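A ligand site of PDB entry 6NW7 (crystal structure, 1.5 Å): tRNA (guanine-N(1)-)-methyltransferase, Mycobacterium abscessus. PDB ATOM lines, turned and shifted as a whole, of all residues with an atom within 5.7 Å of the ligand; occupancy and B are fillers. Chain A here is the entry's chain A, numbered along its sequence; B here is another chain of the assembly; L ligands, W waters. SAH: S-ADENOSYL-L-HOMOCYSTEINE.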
ATOM      1  N   PRO A  85     -11.680 -24.915 -27.544  1.00  0.00           N
ATOM      2  CA  PRO A  85     -11.293 -23.522 -27.275  1.00  0.00           C
ATOM      3  C   PRO A  85      -9.876 -23.417 -26.696  1.00  0.00           C
ATOM      4  O   PRO A  85      -9.469 -24.220 -25.837  1.00  0.00           O
ATOM      5  CB  PRO A  85     -12.343 -23.047 -26.242  1.00  0.00           C
ATOM      6  CG  PRO A  85     -13.494 -24.005 -26.379  1.00  0.00           C
ATOM      7  CD  PRO A  85     -12.900 -25.325 -26.816  1.00  0.00           C
ATOM      8  N   THR A  86      -9.112 -22.455 -27.200  1.00  0.00           N
ATOM      9  CA  THR A  86      -7.758 -22.178 -26.691  1.00  0.00           C
ATOM     10  C   THR A  86      -7.320 -20.778 -27.128  1.00  0.00           C
ATOM     11  O   THR A  86      -7.603 -20.378 -28.262  1.00  0.00           O
ATOM     12  CB  THR A  86      -6.710 -23.233 -27.167  1.00  0.00           C
ATOM     13  OG1 THR A  86      -5.397 -22.715 -26.961  1.00  0.00           O
ATOM     14  CG2 THR A  86      -6.886 -23.613 -28.630  1.00  0.00           C
ATOM     15  N   PRO A  87      -6.651 -20.030 -26.229  1.00  0.00           N
ATOM     16  CA  PRO A  87      -6.170 -18.699 -26.634  1.00  0.00           C
ATOM     17  C   PRO A  87      -5.076 -18.790 -27.717  1.00  0.00           C
ATOM     18  O   PRO A  87      -4.727 -17.775 -28.318  1.00  0.00           O
ATOM     19  CB  PRO A  87      -5.601 -18.102 -25.332  1.00  0.00           C
ATOM     20  CG  PRO A  87      -5.197 -19.315 -24.519  1.00  0.00           C
ATOM     21  CD  PRO A  87      -6.242 -20.379 -24.850  1.00  0.00           C
ATOM     22  N   ALA A  88      -4.526 -19.994 -27.935  1.00  0.00           N
ATOM     23  CA  ALA A  88      -3.561 -20.198 -29.019  1.00  0.00           C
ATOM     24  C   ALA A  88      -4.204 -20.754 -30.291  1.00  0.00           C
ATOM     25  O   ALA A  88      -3.510 -21.247 -31.185  1.00  0.00           O
ATOM     26  CB  ALA A  88      -2.431 -21.150 -28.555  1.00  0.00           C
ATOM     27  N   ALA A 109     -14.939 -29.259 -26.183  1.00  0.00           N
ATOM     28  CA  ALA A 109     -14.069 -29.775 -25.115  1.00  0.00           C
ATOM     29  C   ALA A 109     -13.494 -28.616 -24.314  1.00  0.00           C
ATOM     30  O   ALA A 109     -12.554 -27.961 -24.761  1.00  0.00           O
ATOM     31  CB  ALA A 109     -12.936 -30.617 -25.705  1.00  0.00           C
ATOM     32  N   CYS A 110     -14.028 -28.366 -23.107  1.00  0.00           N
ATOM     33  CA  CYS A 110     -13.636 -27.197 -22.309  1.00  0.00           C
ATOM     34  C   CYS A 110     -12.423 -27.463 -21.415  1.00  0.00           C
ATOM     35  O   CYS A 110     -12.463 -28.309 -20.526  1.00  0.00           O
ATOM     36  CB  CYS A 110     -14.799 -26.715 -21.412  1.00  0.00           C
ATOM     37  SG  CYS A 110     -16.326 -26.220 -22.285  1.00  0.00           S
ATOM     38  N   GLY A 111     -11.337 -26.735 -21.674  1.00  0.00           N
ATOM     39  CA  GLY A 111     -10.129 -26.877 -20.884  1.00  0.00           C
ATOM     40  C   GLY A 111     -10.087 -26.009 -19.633  1.00  0.00           C
ATOM     41  O   GLY A 111     -10.850 -25.044 -19.493  1.00  0.00           O
ATOM     42  N   ARG A 112      -9.206 -26.375 -18.712  1.00  0.00           N
ATOM     43  CA  ARG A 112      -8.863 -25.582 -17.529  1.00  0.00           C
ATOM     44  C   ARG A 112      -7.340 -25.685 -17.319  1.00  0.00           C
ATOM     45  O   ARG A 112      -6.662 -26.427 -18.039  1.00  0.00           O
ATOM     46  CB  ARG A 112      -9.625 -26.063 -16.285  1.00  0.00           C
ATOM     47  CG  ARG A 112     -11.120 -25.673 -16.244  1.00  0.00           C
ATOM     48  CD  ARG A 112     -11.339 -24.377 -15.448  1.00  0.00           C
ATOM     49  NE  ARG A 112     -12.586 -23.714 -15.796  1.00  0.00           N
ATOM     50  CZ  ARG A 112     -13.016 -22.597 -15.211  1.00  0.00           C
ATOM     51  NH1 ARG A 112     -12.302 -22.038 -14.242  1.00  0.00           N
ATOM     52  NH2 ARG A 112     -14.170 -22.046 -15.589  1.00  0.00           N
ATOM     53  N   TYR A 113      -6.817 -24.939 -16.350  1.00  0.00           N
ATOM     54  CA  TYR A 113      -5.384 -24.953 -16.030  1.00  0.00           C
ATOM     55  C   TYR A 113      -4.576 -24.538 -17.265  1.00  0.00           C
ATOM     56  O   TYR A 113      -4.892 -23.521 -17.872  1.00  0.00           O
ATOM     57  CB  TYR A 113      -5.003 -26.346 -15.506  1.00  0.00           C
ATOM     58  CG  TYR A 113      -6.024 -26.801 -14.488  1.00  0.00           C
ATOM     59  CD1 TYR A 113      -6.391 -25.953 -13.440  1.00  0.00           C
ATOM     60  CD2 TYR A 113      -6.670 -28.012 -14.611  1.00  0.00           C
ATOM     61  CE1 TYR A 113      -7.346 -26.346 -12.517  1.00  0.00           C
ATOM     62  CE2 TYR A 113      -7.629 -28.406 -13.698  1.00  0.00           C
ATOM     63  CZ  TYR A 113      -7.965 -27.568 -12.652  1.00  0.00           C
ATOM     64  OH  TYR A 113      -8.910 -27.941 -11.725  1.00  0.00           O
ATOM     65  N   GLU A 114      -3.531 -25.283 -17.636  1.00  0.00           N
ATOM     66  CA  GLU A 114      -2.761 -24.906 -18.814  1.00  0.00           C
ATOM     67  C   GLU A 114      -3.363 -25.440 -20.120  1.00  0.00           C
ATOM     68  O   GLU A 114      -2.836 -25.158 -21.203  1.00  0.00           O
ATOM     69  CB  GLU A 114      -1.311 -25.401 -18.697  1.00  0.00           C
ATOM     70  CG  GLU A 114      -0.558 -24.795 -17.518  1.00  0.00           C
ATOM     71  CD  GLU A 114      -0.349 -23.300 -17.658  1.00  0.00           C
ATOM     72  OE1 GLU A 114      -1.088 -22.525 -17.002  1.00  0.00           O
ATOM     73  OE2 GLU A 114       0.544 -22.902 -18.429  1.00  0.00           O
ATOM     74  N   GLY A 115      -4.462 -26.182 -20.043  1.00  0.00           N
ATOM     75  CA  GLY A 115      -5.088 -26.769 -21.218  1.00  0.00           C
ATOM     76  C   GLY A 115      -4.959 -28.289 -21.271  1.00  0.00           C
ATOM     77  O   GLY A 115      -4.564 -28.919 -20.306  1.00  0.00           O
ATOM     78  N   ILE A 116      -5.323 -28.860 -22.418  1.00  0.00           N
ATOM     79  CA  ILE A 116      -5.380 -30.320 -22.613  1.00  0.00           C
ATOM     80  C   ILE A 116      -4.111 -30.827 -23.290  1.00  0.00           C
ATOM     81  O   ILE A 116      -3.634 -30.205 -24.248  1.00  0.00           O
ATOM     82  CB  ILE A 116      -6.619 -30.692 -23.466  1.00  0.00           C
ATOM     83  CG1 ILE A 116      -7.906 -30.127 -22.833  1.00  0.00           C
ATOM     84  CG2 ILE A 116      -6.750 -32.210 -23.641  1.00  0.00           C
ATOM     85  CD1 ILE A 116      -9.155 -30.302 -23.685  1.00  0.00           C
ATOM     86  N   VAL A 133      -9.735 -23.095 -31.564  1.00  0.00           N
ATOM     87  CA  VAL A 133     -10.118 -21.703 -31.818  1.00  0.00           C
ATOM     88  C   VAL A 133     -10.056 -20.802 -30.581  1.00  0.00           C
ATOM     89  O   VAL A 133     -10.358 -21.234 -29.453  1.00  0.00           O
ATOM     90  CB  VAL A 133     -11.571 -21.582 -32.399  1.00  0.00           C
ATOM     91  CG1 VAL A 133     -11.668 -22.244 -33.785  1.00  0.00           C
ATOM     92  CG2 VAL A 133     -12.629 -22.173 -31.445  1.00  0.00           C
ATOM     93  N   SER A 134      -9.652 -19.552 -30.816  1.00  0.00           N
ATOM     94  CA  SER A 134      -9.688 -18.480 -29.810  1.00  0.00           C
ATOM     95  C   SER A 134     -10.876 -17.552 -30.032  1.00  0.00           C
ATOM     96  O   SER A 134     -11.170 -17.195 -31.177  1.00  0.00           O
ATOM     97  CB  SER A 134      -8.394 -17.656 -29.891  1.00  0.00           C
ATOM     98  OG  SER A 134      -8.507 -16.476 -29.087  1.00  0.00           O
ATOM     99  N   ILE A 135     -11.558 -17.131 -28.955  1.00  0.00           N
ATOM    100  CA  ILE A 135     -12.670 -16.167 -29.117  1.00  0.00           C
ATOM    101  C   ILE A 135     -12.253 -14.696 -28.962  1.00  0.00           C
ATOM    102  O   ILE A 135     -13.096 -13.796 -29.111  1.00  0.00           O
ATOM    103  CB  ILE A 135     -13.862 -16.439 -28.130  1.00  0.00           C
ATOM    104  CG1 ILE A 135     -13.467 -16.272 -26.655  1.00  0.00           C
ATOM    105  CG2 ILE A 135     -14.450 -17.837 -28.402  1.00  0.00           C
ATOM    106  CD1 ILE A 135     -14.687 -15.942 -25.744  1.00  0.00           C
ATOM    107  N   GLY A 136     -10.979 -14.441 -28.702  1.00  0.00           N
ATOM    108  CA  GLY A 136     -10.470 -13.068 -28.646  1.00  0.00           C
ATOM    109  C   GLY A 136      -9.075 -12.975 -28.054  1.00  0.00           C
ATOM    110  O   GLY A 136      -8.553 -13.953 -27.518  1.00  0.00           O
ATOM    111  N   ASP A 137      -8.471 -11.787 -28.142  1.00  0.00           N
ATOM    112  CA  ASP A 137      -7.085 -11.614 -27.702  1.00  0.00           C
ATOM    113  C   ASP A 137      -6.986 -11.240 -26.223  1.00  0.00           C
ATOM    114  O   ASP A 137      -6.528 -10.152 -25.848  1.00  0.00           O
ATOM    115  CB  ASP A 137      -6.376 -10.560 -28.560  1.00  0.00           C
ATOM    116  CG  ASP A 137      -6.144 -11.038 -29.982  1.00  0.00           C
ATOM    117  OD1 ASP A 137      -6.210 -12.265 -30.203  1.00  0.00           O
ATOM    118  OD2 ASP A 137      -5.860 -10.199 -30.865  1.00  0.00           O
ATOM    119  N   TYR A 138      -7.401 -12.196 -25.397  1.00  0.00           N
ATOM    120  CA  TYR A 138      -7.359 -12.103 -23.943  1.00  0.00           C
ATOM    121  C   TYR A 138      -7.302 -13.535 -23.404  1.00  0.00           C
ATOM    122  O   TYR A 138      -7.555 -14.505 -24.150  1.00  0.00           O
ATOM    123  CB  TYR A 138      -8.579 -11.329 -23.381  1.00  0.00           C
ATOM    124  CG  TYR A 138      -9.875 -11.638 -24.103  1.00  0.00           C
ATOM    125  CD1 TYR A 138     -10.541 -12.843 -23.872  1.00  0.00           C
ATOM    126  CD2 TYR A 138     -10.427 -10.756 -25.026  1.00  0.00           C
ATOM    127  CE1 TYR A 138     -11.705 -13.167 -24.544  1.00  0.00           C
ATOM    128  CE2 TYR A 138     -11.601 -11.068 -25.706  1.00  0.00           C
ATOM    129  CZ  TYR A 138     -12.240 -12.286 -25.452  1.00  0.00           C
ATOM    130  OH  TYR A 138     -13.410 -12.628 -26.120  1.00  0.00           O
ATOM    131  N   VAL A 139      -6.973 -13.662 -22.127  1.00  0.00           N
ATOM    132  CA  VAL A 139      -6.836 -14.959 -21.476  1.00  0.00           C
ATOM    133  C   VAL A 139      -7.968 -15.175 -20.457  1.00  0.00           C
ATOM    134  O   VAL A 139      -8.116 -14.407 -19.504  1.00  0.00           O
ATOM    135  CB  VAL A 139      -5.473 -15.102 -20.759  1.00  0.00           C
ATOM    136  CG1 VAL A 139      -5.373 -16.451 -20.062  1.00  0.00           C
ATOM    137  CG2 VAL A 139      -4.339 -14.925 -21.762  1.00  0.00           C
ATOM    138  N   LEU A 140      -8.754 -16.232 -20.679  1.00  0.00           N
ATOM    139  CA  LEU A 140      -9.781 -16.660 -19.728  1.00  0.00           C
ATOM    140  C   LEU A 140      -9.227 -17.687 -18.743  1.00  0.00           C
ATOM    141  O   LEU A 140      -8.144 -18.236 -18.945  1.00  0.00           O
ATOM    142  CB  LEU A 140     -10.971 -17.269 -20.485  1.00  0.00           C
ATOM    143  CG  LEU A 140     -11.635 -16.393 -21.554  1.00  0.00           C
ATOM    144  CD1 LEU A 140     -12.629 -17.204 -22.367  1.00  0.00           C
ATOM    145  CD2 LEU A 140     -12.304 -15.171 -20.924  1.00  0.00           C
ATOM    146  N   ASN A 141      -9.986 -17.971 -17.683  1.00  0.00           N
ATOM    147  CA  ASN A 141      -9.599 -19.030 -16.759  1.00  0.00           C
ATOM    148  C   ASN A 141      -9.970 -20.443 -17.244  1.00  0.00           C
ATOM    149  O   ASN A 141      -9.316 -21.415 -16.895  1.00  0.00           O
ATOM    150  CB  ASN A 141     -10.238 -18.780 -15.390  1.00  0.00           C
ATOM    151  CG  ASN A 141      -9.268 -18.983 -14.254  1.00  0.00           C
ATOM    152  OD1 ASN A 141      -8.415 -18.133 -14.004  1.00  0.00           O
ATOM    153  ND2 ASN A 141      -9.380 -20.109 -13.562  1.00  0.00           N
ATOM    154  N   GLY A 142     -11.021 -20.547 -18.055  1.00  0.00           N
ATOM    155  CA  GLY A 142     -11.449 -21.835 -18.576  1.00  0.00           C
ATOM    156  C   GLY A 142     -12.223 -21.714 -19.884  1.00  0.00           C
ATOM    157  O   GLY A 142     -12.587 -20.602 -20.312  1.00  0.00           O
ATOM    158  N   GLY A 143     -12.494 -22.851 -20.510  1.00  0.00           N
ATOM    159  CA  GLY A 143     -13.216 -22.865 -21.781  1.00  0.00           C
ATOM    160  C   GLY A 143     -14.732 -22.706 -21.700  1.00  0.00           C
ATOM    161  O   GLY A 143     -15.379 -22.574 -22.747  1.00  0.00           O
ATOM    162  N   ALA A 146     -16.040 -19.479 -23.147  1.00  0.00           N
ATOM    163  CA  ALA A 146     -15.848 -19.553 -24.591  1.00  0.00           C
ATOM    164  C   ALA A 146     -16.929 -20.416 -25.255  1.00  0.00           C
ATOM    165  O   ALA A 146     -17.442 -20.072 -26.328  1.00  0.00           O
ATOM    166  CB  ALA A 146     -14.435 -20.118 -24.928  1.00  0.00           C
ATOM    167  N   GLU B 182       1.137 -19.491 -27.055  1.00  0.00           N
ATOM    168  CA  GLU B 182       1.762 -20.608 -26.361  1.00  0.00           C
ATOM    169  C   GLU B 182       1.733 -21.879 -27.219  1.00  0.00           C
ATOM    170  O   GLU B 182       0.763 -22.133 -27.938  1.00  0.00           O
ATOM    171  CB  GLU B 182       1.050 -20.887 -25.033  1.00  0.00           C
ATOM    172  CG  GLU B 182       1.201 -19.786 -23.998  1.00  0.00           C
ATOM    173  CD  GLU B 182       2.157 -20.166 -22.889  1.00  0.00           C
ATOM    174  OE1 GLU B 182       3.373 -19.970 -23.062  1.00  0.00           O
ATOM    175  OE2 GLU B 182       1.684 -20.668 -21.847  1.00  0.00           O
ATOM    176  N   GLY B 183       2.800 -22.662 -27.149  1.00  0.00           N
ATOM    177  CA  GLY B 183       2.833 -23.933 -27.859  1.00  0.00           C
ATOM    178  C   GLY B 183       2.196 -25.043 -27.050  1.00  0.00           C
ATOM    179  O   GLY B 183       1.584 -24.806 -26.017  1.00  0.00           O
HETATM  180  N   SAH L   1      -1.113 -21.764 -21.155  1.00  0.00           N
HETATM  181  CA  SAH L   1      -2.405 -21.954 -21.794  1.00  0.00           C
HETATM  182  CB  SAH L   1      -3.485 -21.263 -20.987  1.00  0.00           C
HETATM  183  CG  SAH L   1      -4.826 -21.996 -20.940  1.00  0.00           C
HETATM  184  SD  SAH L   1      -6.140 -20.911 -20.328  1.00  0.00           S
HETATM  185  C   SAH L   1      -2.385 -21.413 -23.226  1.00  0.00           C
HETATM  186  O   SAH L   1      -2.000 -20.265 -23.461  1.00  0.00           O
HETATM  187  OXT SAH L   1      -2.761 -22.109 -24.172  1.00  0.00           O
HETATM  188  C5' SAH L   1      -7.209 -22.286 -19.814  1.00  0.00           C
HETATM  189  C4' SAH L   1      -8.360 -22.603 -20.762  1.00  0.00           C
HETATM  190  O4' SAH L   1      -9.234 -21.476 -20.903  1.00  0.00           O
HETATM  191  C3' SAH L   1      -7.949 -22.952 -22.187  1.00  0.00           C
HETATM  192  O3' SAH L   1      -7.541 -24.303 -22.351  1.00  0.00           O
HETATM  193  C2' SAH L   1      -9.173 -22.636 -22.992  1.00  0.00           C
HETATM  194  O2' SAH L   1     -10.128 -23.685 -22.854  1.00  0.00           O
HETATM  195  C1' SAH L   1      -9.721 -21.448 -22.236  1.00  0.00           C
HETATM  196  N9  SAH L   1      -9.370 -20.114 -22.814  1.00  0.00           N
HETATM  197  C8  SAH L   1      -8.602 -19.128 -22.239  1.00  0.00           C
HETATM  198  N7  SAH L   1      -8.546 -18.061 -23.086  1.00  0.00           N
HETATM  199  C5  SAH L   1      -9.280 -18.361 -24.192  1.00  0.00           C
HETATM  200  C6  SAH L   1      -9.574 -17.658 -25.371  1.00  0.00           C
HETATM  201  N6  SAH L   1      -9.107 -16.417 -25.612  1.00  0.00           N
HETATM  202  N1  SAH L   1     -10.352 -18.280 -26.323  1.00  0.00           N
HETATM  203  C2  SAH L   1     -10.836 -19.562 -26.136  1.00  0.00           C
HETATM  204  N3  SAH L   1     -10.570 -20.252 -24.978  1.00  0.00           N
HETATM  205  C4  SAH L   1      -9.788 -19.652 -24.025  1.00  0.00           C
HETATM  206  O   HOH W   1     -10.289 -26.375 -24.391  1.00  0.00           O
HETATM  207  O   HOH W   2      -1.475 -18.663 -25.910  1.00  0.00           O
HETATM  208  O   HOH W   3      -7.661 -26.658 -23.762  1.00  0.00           O
HETATM  209  O   HOH W   4      -5.516 -24.691 -24.099  1.00  0.00           O
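The backbone carbonyl oxygen (O) of Gly 136 lies within hydrogen-bond range of a nitrogen (N6) of the ligand (3.2 Å).
N1 of the ligand is in hydrogen-bond range of N of Ile 135.
An oxygen (O2') of the ligand sits close to the backbone NH (N) of Gly 143 (3.4 Å).
An oxygen (O4') of the ligand sits close to the backbone NH (N) of Gly 142.
A nitrogen (N) of the ligand lies within salt-bridge range of the side-chain carboxylate of Glu 114 (3.4 Å).
The backbone carbonyl oxygen (O) of Tyr 138 lies within hydrogen-bond range of a nitrogen (N6) of the ligand (2.9 Å).
The backbone NH (N) of Thr 86 lies within hydrogen-bond range of a nitrogen (N3) of the ligand (3.5 Å).
O2' of the ligand sits at hydrogen-bond distance from N of Gly 111 (3.5 Å).
The backbone NH (N) of Leu 140 sits at hydrogen-bond distance from a nitrogen (N7) of the ligand, at 3.0 Å.
The side-chain carboxylate of Glu 182 of chain B lies within salt-bridge range of a nitrogen (N) of the ligand (3.1 Å).
The backbone carbonyl oxygen (O) of Pro 85 sits at hydrogen-bond distance from an oxygen (O2') of the ligand (3.1 Å).
The backbone NH (N) of Ala 88 lies close to the side-chain hydroxyl (OG1) of Thr 86 (3.0 Å).
The backbone carbonyl oxygen of Val 133 is in hydrogen-bond range of the backbone NH of Thr 86 (2.8 Å).
O of Gly 136 lies within hydrogen-bond range of OG of Ser 134.
The side-chain hydroxyl of Tyr 138 is in hydrogen-bond range of the backbone carbonyl oxygen of Ile 135.
O of Gly 143 is in hydrogen-bond range of SG of Cys 110, 3.8 Å away.
The backbone carbonyl oxygen (O) of Thr 86 lies close to the backbone NH (N) of Ser 134.
N of Gly 143 sits at hydrogen-bond distance from O of Gly 111.
The backbone carbonyl oxygen of Tyr 113 lies close to a sulfur (SD) of the ligand.
Pro 87 touches the ligand.
CA of Gly 115 touches O3' of the ligand, at 3.7 Å.
O of Val 133 touches C2 of the ligand, at 3.7 Å.
OG of Ser 134 touches N6 of the ligand, 3.5 Å away.
Val 139 touches the ligand (CA to N7, 3.9 Å).
Asn 141 touches the ligand (O to C5', 3.7 Å).
CB of Ala 146 touches C2 of the ligand, 3.8 Å away.
Water W4 lies within hydrogen-bond range of O3' of the ligand and OG1 of Thr 86.
Water W3 lies within hydrogen-bond range of an oxygen (O3') of the ligand and the backbone NH of Ile 116.
Water W2 lies within hydrogen-bond range of N of Glu 182 of chain B (3.0 Å) and O of the ligand (3.0 Å).
Water W1 lies within hydrogen-bond range of O of Pro 85, O of Ala 109, N of Gly 111 and O2' of the ligand.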
